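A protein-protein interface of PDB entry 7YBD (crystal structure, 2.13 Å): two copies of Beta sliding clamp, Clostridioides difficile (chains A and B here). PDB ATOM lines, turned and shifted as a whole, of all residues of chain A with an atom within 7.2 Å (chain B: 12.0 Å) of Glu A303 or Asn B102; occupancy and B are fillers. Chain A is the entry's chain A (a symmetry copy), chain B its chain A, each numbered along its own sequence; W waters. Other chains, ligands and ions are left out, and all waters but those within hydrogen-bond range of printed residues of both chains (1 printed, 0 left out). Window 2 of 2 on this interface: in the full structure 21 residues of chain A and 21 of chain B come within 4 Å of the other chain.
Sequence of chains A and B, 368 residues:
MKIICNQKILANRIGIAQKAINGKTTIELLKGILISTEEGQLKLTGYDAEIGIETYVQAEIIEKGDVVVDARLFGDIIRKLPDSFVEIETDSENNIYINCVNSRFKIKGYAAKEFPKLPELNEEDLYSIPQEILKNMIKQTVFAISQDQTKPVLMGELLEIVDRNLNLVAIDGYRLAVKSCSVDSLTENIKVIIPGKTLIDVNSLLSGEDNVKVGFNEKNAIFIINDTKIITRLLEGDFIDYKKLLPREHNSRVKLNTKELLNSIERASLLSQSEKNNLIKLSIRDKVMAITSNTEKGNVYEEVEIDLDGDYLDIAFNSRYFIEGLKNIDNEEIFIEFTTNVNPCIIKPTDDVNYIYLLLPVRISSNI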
ATOM      1  N   GLU A 260      -6.728  -3.414   6.296  1.00  0.00           N
ATOM      2  CA  GLU A 260      -7.912  -2.989   5.572  1.00  0.00           C
ATOM      3  C   GLU A 260      -8.706  -4.207   5.116  1.00  0.00           C
ATOM      4  O   GLU A 260      -9.907  -4.262   5.319  1.00  0.00           O
ATOM      5  CB  GLU A 260      -7.559  -2.091   4.395  1.00  0.00           C
ATOM      6  CG  GLU A 260      -7.361  -0.664   4.839  1.00  0.00           C
ATOM      7  CD  GLU A 260      -6.795   0.243   3.760  1.00  0.00           C
ATOM      8  OE1 GLU A 260      -6.236   1.305   4.134  1.00  0.00           O
ATOM      9  OE2 GLU A 260      -6.906  -0.109   2.543  1.00  0.00           O
ATOM     10  N   SER A 264     -12.543  -5.408   6.681  1.00  0.00           N
ATOM     11  CA  SER A 264     -13.642  -5.609   5.742  1.00  0.00           C
ATOM     12  C   SER A 264     -14.174  -7.036   5.806  1.00  0.00           C
ATOM     13  O   SER A 264     -15.384  -7.248   5.848  1.00  0.00           O
ATOM     14  CB  SER A 264     -13.241  -5.256   4.340  1.00  0.00           C
ATOM     15  OG  SER A 264     -12.978  -3.870   4.264  1.00  0.00           O
ATOM     16  N   ARG A 267     -16.173  -7.337   9.047  1.00  0.00           N
ATOM     17  CA  ARG A 267     -17.490  -6.735   8.922  1.00  0.00           C
ATOM     18  C   ARG A 267     -18.399  -7.613   8.054  1.00  0.00           C
ATOM     19  O   ARG A 267     -19.517  -7.929   8.454  1.00  0.00           O
ATOM     20  CB  ARG A 267     -17.348  -5.273   8.476  1.00  0.00           C
ATOM     21  CG  ARG A 267     -16.883  -4.366   9.614  1.00  0.00           C
ATOM     22  CD  ARG A 267     -16.920  -2.902   9.235  1.00  0.00           C
ATOM     23  NE  ARG A 267     -16.051  -2.543   8.124  1.00  0.00           N
ATOM     24  CZ  ARG A 267     -14.810  -2.082   8.252  1.00  0.00           C
ATOM     25  NH1 ARG A 267     -14.267  -1.930   9.448  1.00  0.00           N
ATOM     26  NH2 ARG A 267     -14.107  -1.788   7.176  1.00  0.00           N
ATOM     27  N   VAL A 288     -10.276  -1.302  -7.028  1.00  0.00           N
ATOM     28  CA  VAL A 288     -11.125  -1.646  -5.890  1.00  0.00           C
ATOM     29  C   VAL A 288     -11.383  -3.158  -5.873  1.00  0.00           C
ATOM     30  O   VAL A 288     -11.581  -3.777  -6.914  1.00  0.00           O
ATOM     31  CB  VAL A 288     -12.461  -0.868  -5.928  1.00  0.00           C
ATOM     32  CG1 VAL A 288     -13.376  -1.190  -4.751  1.00  0.00           C
ATOM     33  CG2 VAL A 288     -12.249   0.634  -6.026  1.00  0.00           C
ATOM     34  N   MET A 289     -11.383  -3.751  -4.675  1.00  0.00           N
ATOM     35  CA  MET A 289     -11.936  -5.081  -4.464  1.00  0.00           C
ATOM     36  C   MET A 289     -13.163  -4.928  -3.565  1.00  0.00           C
ATOM     37  O   MET A 289     -13.076  -4.267  -2.527  1.00  0.00           O
ATOM     38  CB  MET A 289     -10.905  -6.011  -3.815  1.00  0.00           C
ATOM     39  CG  MET A 289     -11.399  -7.429  -3.579  1.00  0.00           C
ATOM     40  SD  MET A 289     -10.357  -8.231  -2.317  1.00  0.00           S
ATOM     41  CE  MET A 289      -9.284  -9.169  -3.393  1.00  0.00           C
ATOM     42  N   ALA A 290     -14.310  -5.475  -4.008  1.00  0.00           N
ATOM     43  CA  ALA A 290     -15.514  -5.481  -3.192  1.00  0.00           C
ATOM     44  C   ALA A 290     -15.567  -6.770  -2.374  1.00  0.00           C
ATOM     45  O   ALA A 290     -15.216  -7.844  -2.860  1.00  0.00           O
ATOM     46  CB  ALA A 290     -16.758  -5.267  -4.035  1.00  0.00           C
ATOM     47  N   ILE A 291     -15.998  -6.655  -1.121  1.00  0.00           N
ATOM     48  CA  ILE A 291     -16.184  -7.829  -0.278  1.00  0.00           C
ATOM     49  C   ILE A 291     -17.649  -7.817   0.160  1.00  0.00           C
ATOM     50  O   ILE A 291     -18.124  -6.841   0.740  1.00  0.00           O
ATOM     51  CB  ILE A 291     -15.208  -7.813   0.930  1.00  0.00           C
ATOM     52  CG1 ILE A 291     -13.738  -7.768   0.506  1.00  0.00           C
ATOM     53  CG2 ILE A 291     -15.474  -8.977   1.872  1.00  0.00           C
ATOM     54  CD1 ILE A 291     -13.187  -6.360   0.327  1.00  0.00           C
ATOM     55  N   TYR A 301     -21.738  -4.627   1.808  1.00  0.00           N
ATOM     56  CA  TYR A 301     -20.878  -4.297   0.694  1.00  0.00           C
ATOM     57  C   TYR A 301     -19.696  -3.515   1.257  1.00  0.00           C
ATOM     58  O   TYR A 301     -19.867  -2.423   1.804  1.00  0.00           O
ATOM     59  CB  TYR A 301     -21.659  -3.464  -0.325  1.00  0.00           C
ATOM     60  CG  TYR A 301     -21.035  -3.458  -1.692  1.00  0.00           C
ATOM     61  CD1 TYR A 301     -19.971  -2.617  -1.980  1.00  0.00           C
ATOM     62  CD2 TYR A 301     -21.485  -4.330  -2.681  1.00  0.00           C
ATOM     63  CE1 TYR A 301     -19.376  -2.624  -3.236  1.00  0.00           C
ATOM     64  CE2 TYR A 301     -20.903  -4.348  -3.940  1.00  0.00           C
ATOM     65  CZ  TYR A 301     -19.848  -3.487  -4.215  1.00  0.00           C
ATOM     66  OH  TYR A 301     -19.277  -3.481  -5.458  1.00  0.00           O
ATOM     67  N   GLU A 302     -18.501  -4.096   1.158  1.00  0.00           N
ATOM     68  CA  GLU A 302     -17.315  -3.422   1.667  1.00  0.00           C
ATOM     69  C   GLU A 302     -16.452  -3.137   0.455  1.00  0.00           C
ATOM     70  O   GLU A 302     -16.479  -3.927  -0.486  1.00  0.00           O
ATOM     71  CB  GLU A 302     -16.521  -4.353   2.594  1.00  0.00           C
ATOM     72  CG  GLU A 302     -17.097  -4.516   3.999  1.00  0.00           C
ATOM     73  CD  GLU A 302     -16.781  -3.375   4.963  1.00  0.00           C
ATOM     74  OE1 GLU A 302     -17.669  -3.065   5.800  1.00  0.00           O
ATOM     75  OE2 GLU A 302     -15.657  -2.792   4.891  1.00  0.00           O
ATOM     76  N   GLU A 303     -15.717  -2.020   0.484  1.00  0.00           N
ATOM     77  CA  GLU A 303     -14.758  -1.740  -0.578  1.00  0.00           C
ATOM     78  C   GLU A 303     -13.359  -1.550  -0.011  1.00  0.00           C
ATOM     79  O   GLU A 303     -13.188  -0.901   1.013  1.00  0.00           O
ATOM     80  CB  GLU A 303     -15.150  -0.500  -1.371  1.00  0.00           C
ATOM     81  CG  GLU A 303     -16.200  -0.851  -2.403  1.00  0.00           C
ATOM     82  CD  GLU A 303     -16.733   0.339  -3.170  1.00  0.00           C
ATOM     83  OE1 GLU A 303     -17.062   0.168  -4.362  1.00  0.00           O
ATOM     84  OE2 GLU A 303     -16.827   1.420  -2.565  1.00  0.00           O
ATOM     85  N   VAL A 304     -12.370  -2.113  -0.710  1.00  0.00           N
ATOM     86  CA  VAL A 304     -10.976  -1.994  -0.317  1.00  0.00           C
ATOM     87  C   VAL A 304     -10.163  -1.623  -1.562  1.00  0.00           C
ATOM     88  O   VAL A 304     -10.340  -2.196  -2.639  1.00  0.00           O
ATOM     89  CB  VAL A 304     -10.505  -3.308   0.341  1.00  0.00           C
ATOM     90  CG1 VAL A 304      -9.005  -3.519   0.250  1.00  0.00           C
ATOM     91  CG2 VAL A 304     -10.977  -3.408   1.787  1.00  0.00           C
ATOM     92  N   GLU A 305      -9.280  -0.644  -1.398  1.00  0.00           N
ATOM     93  CA  GLU A 305      -8.466  -0.121  -2.476  1.00  0.00           C
ATOM     94  C   GLU A 305      -7.433  -1.186  -2.850  1.00  0.00           C
ATOM     95  O   GLU A 305      -6.872  -1.805  -1.953  1.00  0.00           O
ATOM     96  CB  GLU A 305      -7.821   1.155  -1.926  1.00  0.00           C
ATOM     97  CG  GLU A 305      -7.054   1.922  -2.972  1.00  0.00           C
ATOM     98  CD  GLU A 305      -6.226   3.074  -2.424  1.00  0.00           C
ATOM     99  OE1 GLU A 305      -5.090   3.255  -2.904  1.00  0.00           O
ATOM    100  OE2 GLU A 305      -6.726   3.797  -1.536  1.00  0.00           O
ATOM    101  N   GLN B   7     -19.639   7.360  15.114  1.00  0.00           N
ATOM    102  CA  GLN B   7     -19.510   5.930  15.378  1.00  0.00           C
ATOM    103  C   GLN B   7     -19.206   5.605  16.845  1.00  0.00           C
ATOM    104  O   GLN B   7     -19.727   4.614  17.364  1.00  0.00           O
ATOM    105  CB  GLN B   7     -18.397   5.292  14.549  1.00  0.00           C
ATOM    106  CG  GLN B   7     -18.212   3.815  14.862  1.00  0.00           C
ATOM    107  CD  GLN B   7     -17.115   3.544  15.865  1.00  0.00           C
ATOM    108  OE1 GLN B   7     -16.270   4.387  16.156  1.00  0.00           O
ATOM    109  NE2 GLN B   7     -17.091   2.331  16.385  1.00  0.00           N
ATOM    110  N   ILE B  77     -22.049  -4.602  14.557  1.00  0.00           N
ATOM    111  CA  ILE B  77     -21.710  -3.808  13.383  1.00  0.00           C
ATOM    112  C   ILE B  77     -21.037  -2.502  13.811  1.00  0.00           C
ATOM    113  O   ILE B  77     -19.940  -2.178  13.341  1.00  0.00           O
ATOM    114  CB  ILE B  77     -22.962  -3.549  12.510  1.00  0.00           C
ATOM    115  CG1 ILE B  77     -23.410  -4.827  11.790  1.00  0.00           C
ATOM    116  CG2 ILE B  77     -22.721  -2.391  11.541  1.00  0.00           C
ATOM    117  CD1 ILE B  77     -24.837  -4.793  11.253  1.00  0.00           C
ATOM    118  N   LYS B  80     -17.394  -2.402  14.977  1.00  0.00           N
ATOM    119  CA  LYS B  80     -16.319  -2.666  14.022  1.00  0.00           C
ATOM    120  C   LYS B  80     -16.143  -1.550  12.981  1.00  0.00           C
ATOM    121  O   LYS B  80     -15.304  -1.684  12.081  1.00  0.00           O
ATOM    122  CB  LYS B  80     -16.605  -3.936  13.214  1.00  0.00           C
ATOM    123  CG  LYS B  80     -16.416  -5.260  13.936  1.00  0.00           C
ATOM    124  CD  LYS B  80     -14.982  -5.527  14.297  1.00  0.00           C
ATOM    125  CE  LYS B  80     -14.765  -6.915  14.849  1.00  0.00           C
ATOM    126  NZ  LYS B  80     -14.812  -6.874  16.329  1.00  0.00           N
ATOM    127  N   LEU B  81     -16.982  -0.507  13.020  1.00  0.00           N
ATOM    128  CA  LEU B  81     -16.858   0.553  12.028  1.00  0.00           C
ATOM    129  C   LEU B  81     -15.785   1.539  12.468  1.00  0.00           C
ATOM    130  O   LEU B  81     -15.525   1.718  13.652  1.00  0.00           O
ATOM    131  CB  LEU B  81     -18.203   1.255  11.820  1.00  0.00           C
ATOM    132  CG  LEU B  81     -19.310   0.374  11.225  1.00  0.00           C
ATOM    133  CD1 LEU B  81     -20.636   1.126  11.207  1.00  0.00           C
ATOM    134  CD2 LEU B  81     -18.948  -0.105   9.827  1.00  0.00           C
ATOM    135  N   PRO B  82     -15.137   2.227  11.513  1.00  0.00           N
ATOM    136  CA  PRO B  82     -14.102   3.194  11.868  1.00  0.00           C
ATOM    137  C   PRO B  82     -14.749   4.388  12.564  1.00  0.00           C
ATOM    138  O   PRO B  82     -15.960   4.605  12.443  1.00  0.00           O
ATOM    139  CB  PRO B  82     -13.540   3.632  10.512  1.00  0.00           C
ATOM    140  CG  PRO B  82     -14.663   3.331   9.514  1.00  0.00           C
ATOM    141  CD  PRO B  82     -15.401   2.129  10.063  1.00  0.00           C
ATOM    142  N   ASP B  83     -13.907   5.152  13.269  1.00  0.00           N
ATOM    143  CA  ASP B  83     -14.292   6.317  14.041  1.00  0.00           C
ATOM    144  C   ASP B  83     -14.658   7.454  13.089  1.00  0.00           C
ATOM    145  O   ASP B  83     -13.875   8.357  12.848  1.00  0.00           O
ATOM    146  CB  ASP B  83     -13.174   6.713  15.005  1.00  0.00           C
ATOM    147  CG  ASP B  83     -13.504   7.952  15.807  1.00  0.00           C
ATOM    148  OD1 ASP B  83     -14.709   8.304  15.865  1.00  0.00           O
ATOM    149  OD2 ASP B  83     -12.559   8.549  16.379  1.00  0.00           O
ATOM    150  N   SER B  84     -15.849   7.389  12.510  1.00  0.00           N
ATOM    151  CA  SER B  84     -16.238   8.414  11.566  1.00  0.00           C
ATOM    152  C   SER B  84     -17.731   8.640  11.744  1.00  0.00           C
ATOM    153  O   SER B  84     -18.297   8.204  12.754  1.00  0.00           O
ATOM    154  CB  SER B  84     -15.893   8.001  10.134  1.00  0.00           C
ATOM    155  OG  SER B  84     -16.219   9.061   9.228  1.00  0.00           O
ATOM    156  N   PHE B  85     -18.347   9.298  10.753  1.00  0.00           N
ATOM    157  CA  PHE B  85     -19.782   9.496  10.705  1.00  0.00           C
ATOM    158  C   PHE B  85     -20.467   8.197  10.272  1.00  0.00           C
ATOM    159  O   PHE B  85     -19.983   7.499   9.386  1.00  0.00           O
ATOM    160  CB  PHE B  85     -20.088  10.668   9.771  1.00  0.00           C
ATOM    161  CG  PHE B  85     -19.587  11.997  10.289  1.00  0.00           C
ATOM    162  CD1 PHE B  85     -20.149  12.577  11.429  1.00  0.00           C
ATOM    163  CD2 PHE B  85     -18.537  12.663   9.660  1.00  0.00           C
ATOM    164  CE1 PHE B  85     -19.661  13.780  11.922  1.00  0.00           C
ATOM    165  CE2 PHE B  85     -18.064  13.880  10.151  1.00  0.00           C
ATOM    166  CZ  PHE B  85     -18.630  14.441  11.278  1.00  0.00           C
ATOM    167  N   VAL B  86     -21.600   7.877  10.912  1.00  0.00           N
ATOM    168  CA  VAL B  86     -22.448   6.752  10.555  1.00  0.00           C
ATOM    169  C   VAL B  86     -23.818   7.303  10.174  1.00  0.00           C
ATOM    170  O   VAL B  86     -24.477   7.970  10.980  1.00  0.00           O
ATOM    171  CB  VAL B  86     -22.618   5.761  11.730  1.00  0.00           C
ATOM    172  CG1 VAL B  86     -23.513   4.582  11.350  1.00  0.00           C
ATOM    173  CG2 VAL B  86     -21.282   5.271  12.268  1.00  0.00           C
ATOM    174  N   GLU B  87     -24.257   6.932   8.974  1.00  0.00           N
ATOM    175  CA  GLU B  87     -25.581   7.252   8.465  1.00  0.00           C
ATOM    176  C   GLU B  87     -26.488   6.037   8.659  1.00  0.00           C
ATOM    177  O   GLU B  87     -26.103   4.909   8.381  1.00  0.00           O
ATOM    178  CB  GLU B  87     -25.440   7.592   6.982  1.00  0.00           C
ATOM    179  CG  GLU B  87     -26.750   7.864   6.278  1.00  0.00           C
ATOM    180  CD  GLU B  87     -26.554   8.184   4.803  1.00  0.00           C
ATOM    181  OE1 GLU B  87     -27.048   9.241   4.356  1.00  0.00           O
ATOM    182  OE2 GLU B  87     -25.904   7.380   4.110  1.00  0.00           O
ATOM    183  N   TYR B  97     -30.421   0.578   6.732  1.00  0.00           N
ATOM    184  CA  TYR B  97     -29.201   0.795   5.968  1.00  0.00           C
ATOM    185  C   TYR B  97     -28.206   1.531   6.875  1.00  0.00           C
ATOM    186  O   TYR B  97     -28.545   2.558   7.453  1.00  0.00           O
ATOM    187  CB  TYR B  97     -29.550   1.610   4.711  1.00  0.00           C
ATOM    188  CG  TYR B  97     -30.620   0.975   3.848  1.00  0.00           C
ATOM    189  CD1 TYR B  97     -31.970   1.079   4.181  1.00  0.00           C
ATOM    190  CD2 TYR B  97     -30.292   0.238   2.721  1.00  0.00           C
ATOM    191  CE1 TYR B  97     -32.958   0.479   3.413  1.00  0.00           C
ATOM    192  CE2 TYR B  97     -31.272  -0.353   1.931  1.00  0.00           C
ATOM    193  CZ  TYR B  97     -32.610  -0.219   2.269  1.00  0.00           C
ATOM    194  OH  TYR B  97     -33.588  -0.832   1.544  1.00  0.00           O
ATOM    195  N   ILE B  98     -26.995   1.000   7.042  1.00  0.00           N
ATOM    196  CA  ILE B  98     -25.988   1.669   7.851  1.00  0.00           C
ATOM    197  C   ILE B  98     -24.798   1.906   6.934  1.00  0.00           C
ATOM    198  O   ILE B  98     -24.269   0.936   6.399  1.00  0.00           O
ATOM    199  CB  ILE B  98     -25.605   0.757   9.046  1.00  0.00           C
ATOM    200  CG1 ILE B  98     -26.812   0.336   9.902  1.00  0.00           C
ATOM    201  CG2 ILE B  98     -24.508   1.381   9.898  1.00  0.00           C
ATOM    202  CD1 ILE B  98     -26.456  -0.608  11.050  1.00  0.00           C
ATOM    203  N   ASN B  99     -24.367   3.174   6.782  1.00  0.00           N
ATOM    204  CA  ASN B  99     -23.294   3.517   5.858  1.00  0.00           C
ATOM    205  C   ASN B  99     -22.190   4.251   6.598  1.00  0.00           C
ATOM    206  O   ASN B  99     -22.473   5.118   7.416  1.00  0.00           O
ATOM    207  CB  ASN B  99     -23.817   4.373   4.698  1.00  0.00           C
ATOM    208  CG  ASN B  99     -24.863   3.599   3.925  1.00  0.00           C
ATOM    209  OD1 ASN B  99     -24.689   2.409   3.672  1.00  0.00           O
ATOM    210  ND2 ASN B  99     -25.985   4.231   3.624  1.00  0.00           N
ATOM    211  N   CYS B 100     -20.935   3.924   6.305  1.00  0.00           N
ATOM    212  CA  CYS B 100     -19.857   4.570   7.031  1.00  0.00           C
ATOM    213  C   CYS B 100     -18.575   4.300   6.254  1.00  0.00           C
ATOM    214  O   CYS B 100     -18.250   3.131   6.025  1.00  0.00           O
ATOM    215  CB  CYS B 100     -19.798   3.991   8.445  1.00  0.00           C
ATOM    216  SG  CYS B 100     -18.436   4.571   9.496  1.00  0.00           S
ATOM    217  N   VAL B 101     -17.879   5.384   5.871  1.00  0.00           N
ATOM    218  CA  VAL B 101     -16.706   5.354   5.002  1.00  0.00           C
ATOM    219  C   VAL B 101     -16.954   4.340   3.885  1.00  0.00           C
ATOM    220  O   VAL B 101     -17.833   4.530   3.058  1.00  0.00           O
ATOM    221  CB  VAL B 101     -15.395   5.095   5.777  1.00  0.00           C
ATOM    222  CG1 VAL B 101     -14.179   5.488   4.949  1.00  0.00           C
ATOM    223  CG2 VAL B 101     -15.396   5.839   7.097  1.00  0.00           C
ATOM    224  N   ASN B 102     -16.248   3.216   3.878  1.00  0.00           N
ATOM    225  CA  ASN B 102     -16.452   2.350   2.733  1.00  0.00           C
ATOM    226  C   ASN B 102     -17.274   1.107   3.078  1.00  0.00           C
ATOM    227  O   ASN B 102     -17.049   0.051   2.476  1.00  0.00           O
ATOM    228  CB  ASN B 102     -15.112   2.041   2.066  1.00  0.00           C
ATOM    229  CG  ASN B 102     -14.572   3.286   1.404  1.00  0.00           C
ATOM    230  OD1 ASN B 102     -15.240   3.902   0.578  1.00  0.00           O
ATOM    231  ND2 ASN B 102     -13.380   3.681   1.800  1.00  0.00           N
ATOM    232  N   SER B 103     -18.212   1.231   4.038  1.00  0.00           N
ATOM    233  CA  SER B 103     -19.034   0.089   4.446  1.00  0.00           C
ATOM    234  C   SER B 103     -20.496   0.397   4.182  1.00  0.00           C
ATOM    235  O   SER B 103     -20.940   1.472   4.541  1.00  0.00           O
ATOM    236  CB  SER B 103     -18.902  -0.232   5.911  1.00  0.00           C
ATOM    237  OG  SER B 103     -17.584  -0.602   6.217  1.00  0.00           O
ATOM    238  N   ARG B 104     -21.230  -0.574   3.627  1.00  0.00           N
ATOM    239  CA  ARG B 104     -22.666  -0.455   3.411  1.00  0.00           C
ATOM    240  C   ARG B 104     -23.315  -1.753   3.864  1.00  0.00           C
ATOM    241  O   ARG B 104     -22.952  -2.825   3.387  1.00  0.00           O
ATOM    242  CB  ARG B 104     -22.973  -0.176   1.938  1.00  0.00           C
ATOM    243  CG  ARG B 104     -22.519   1.216   1.526  1.00  0.00           C
ATOM    244  CD  ARG B 104     -22.937   1.646   0.139  1.00  0.00           C
ATOM    245  NE  ARG B 104     -22.040   2.646  -0.440  1.00  0.00           N
ATOM    246  CZ  ARG B 104     -22.433   3.696  -1.157  1.00  0.00           C
ATOM    247  NH1 ARG B 104     -23.719   3.899  -1.400  1.00  0.00           N
ATOM    248  NH2 ARG B 104     -21.536   4.543  -1.631  1.00  0.00           N
ATOM    249  N   PHE B 105     -24.193  -1.634   4.861  1.00  0.00           N
ATOM    250  CA  PHE B 105     -24.933  -2.774   5.371  1.00  0.00           C
ATOM    251  C   PHE B 105     -26.397  -2.480   5.120  1.00  0.00           C
ATOM    252  O   PHE B 105     -26.832  -1.314   5.137  1.00  0.00           O
ATOM    253  CB  PHE B 105     -24.829  -2.844   6.890  1.00  0.00           C
ATOM    254  CG  PHE B 105     -23.494  -3.328   7.384  1.00  0.00           C
ATOM    255  CD1 PHE B 105     -22.412  -2.466   7.431  1.00  0.00           C
ATOM    256  CD2 PHE B 105     -23.332  -4.650   7.781  1.00  0.00           C
ATOM    257  CE1 PHE B 105     -21.185  -2.926   7.874  1.00  0.00           C
ATOM    258  CE2 PHE B 105     -22.105  -5.100   8.241  1.00  0.00           C
ATOM    259  CZ  PHE B 105     -21.036  -4.232   8.282  1.00  0.00           C
ATOM    260  N   LYS B 106     -27.120  -3.560   4.846  1.00  0.00           N
ATOM    261  CA  LYS B 106     -28.562  -3.517   4.904  1.00  0.00           C
ATOM    262  C   LYS B 106     -28.998  -4.701   5.763  1.00  0.00           C
ATOM    263  O   LYS B 106     -28.698  -5.838   5.417  1.00  0.00           O
ATOM    264  CB  LYS B 106     -29.147  -3.589   3.495  1.00  0.00           C
ATOM    265  CG  LYS B 106     -30.671  -3.657   3.467  1.00  0.00           C
ATOM    266  CD  LYS B 106     -31.235  -3.800   2.068  1.00  0.00           C
ATOM    267  CE  LYS B 106     -32.733  -3.996   2.031  1.00  0.00           C
ATOM    268  NZ  LYS B 106     -33.117  -4.781   0.841  1.00  0.00           N
HETATM  269  O   HOH W   1     -19.037   0.180   0.460  1.00  0.00           O
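NE of Arg A267 is in hydrogen-bond range of OG of Ser B103 (3.1 Å).
O of Asn B102 lies within hydrogen-bond range of N of Glu A303.
The backbone carbonyl oxygen (O) of Arg B104 is in hydrogen-bond range of the backbone NH (N) of Tyr A301 (2.7 Å).
OG of Ser B103 sits at hydrogen-bond distance from OE1 of Glu A302 (2.5 Å).
NH1 of Arg A267 lies within hydrogen-bond range of O of Lys B80 (2.8 Å).
OE2 of Glu A302 is in hydrogen-bond range of OG of Ser A264 (3.0 Å).
The side-chain amide nitrogen (NE2) of Gln B7 is in hydrogen-bond range of the backbone carbonyl oxygen (O) of Leu B81, 3.2 Å away.
The backbone carbonyl oxygen of Ile B98 is in hydrogen-bond range of the backbone NH of Phe B105, 3.0 Å away.
The backbone carbonyl oxygen (O) of Ile A291 lies within hydrogen-bond range of the backbone NH (N) of Glu A302, 2.8 Å away.
OE1 of Glu A302 is in salt-bridge range of NE of Arg A267 (2.9 Å).
CD of Arg A267 touches CD2 of Leu B81, 3.5 Å away.
Arg A267 touches Phe B105.
O of Tyr A301 touches O of Asn B102 (3.8 Å).
Tyr A301 touches Ser B103.
Glu A302 touches Asn B102.
No residue of chain B comes within 4 Å of Val A288.
No residue of chain B comes within 4 Å of Ala A290.
No residue of chain B comes within 4 Å of Ile A291.
Of chain B, only Asn B102 (3.8 Å), Ser B103 (3.7 Å) and Arg B104 (2.7 Å) come within 4 Å of Tyr A301.
Glu A303 touches just one residue of chain B: Asn B102.
No residue of chain B comes within 4 Å of Val A304.
Of the printed residues of chain A, Leu B81 touches Arg A267 (3.5 Å).
Of chain A, only Tyr A301 (3.8 Å), Glu A302 (3.6 Å) and Glu A303 (3.2 Å) come within 4 Å of Asn B102.
Of the printed residues of chain A, Phe B105 touches Arg A267.
The nearest residue of chain A that does not touch Asn B102 is Val A304 (5.7 Å).
Of the 20 printed residues of chain B, 6 touch a printed residue of chain A.
Printed residues of chain B that touch a printed residue of chain A: Lys B80, Leu B81, Asn B102, Ser B103, Arg B104 and Phe B105.
Hydrophobic or aromatic side chains of chain A within 4 Å of the printed part of chain B: Tyr A301.
Along chain A the printed residues that touch a printed residue of chain B span positions 267 to 303.
Among the printed residues, no Asp or Glu carboxylate lies within 4 Å of a Lys or Arg side-chain nitrogen of the other chain.
No position is printed for both chains.
Water W1 bridges O of Asn B102 and O of Tyr A301.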
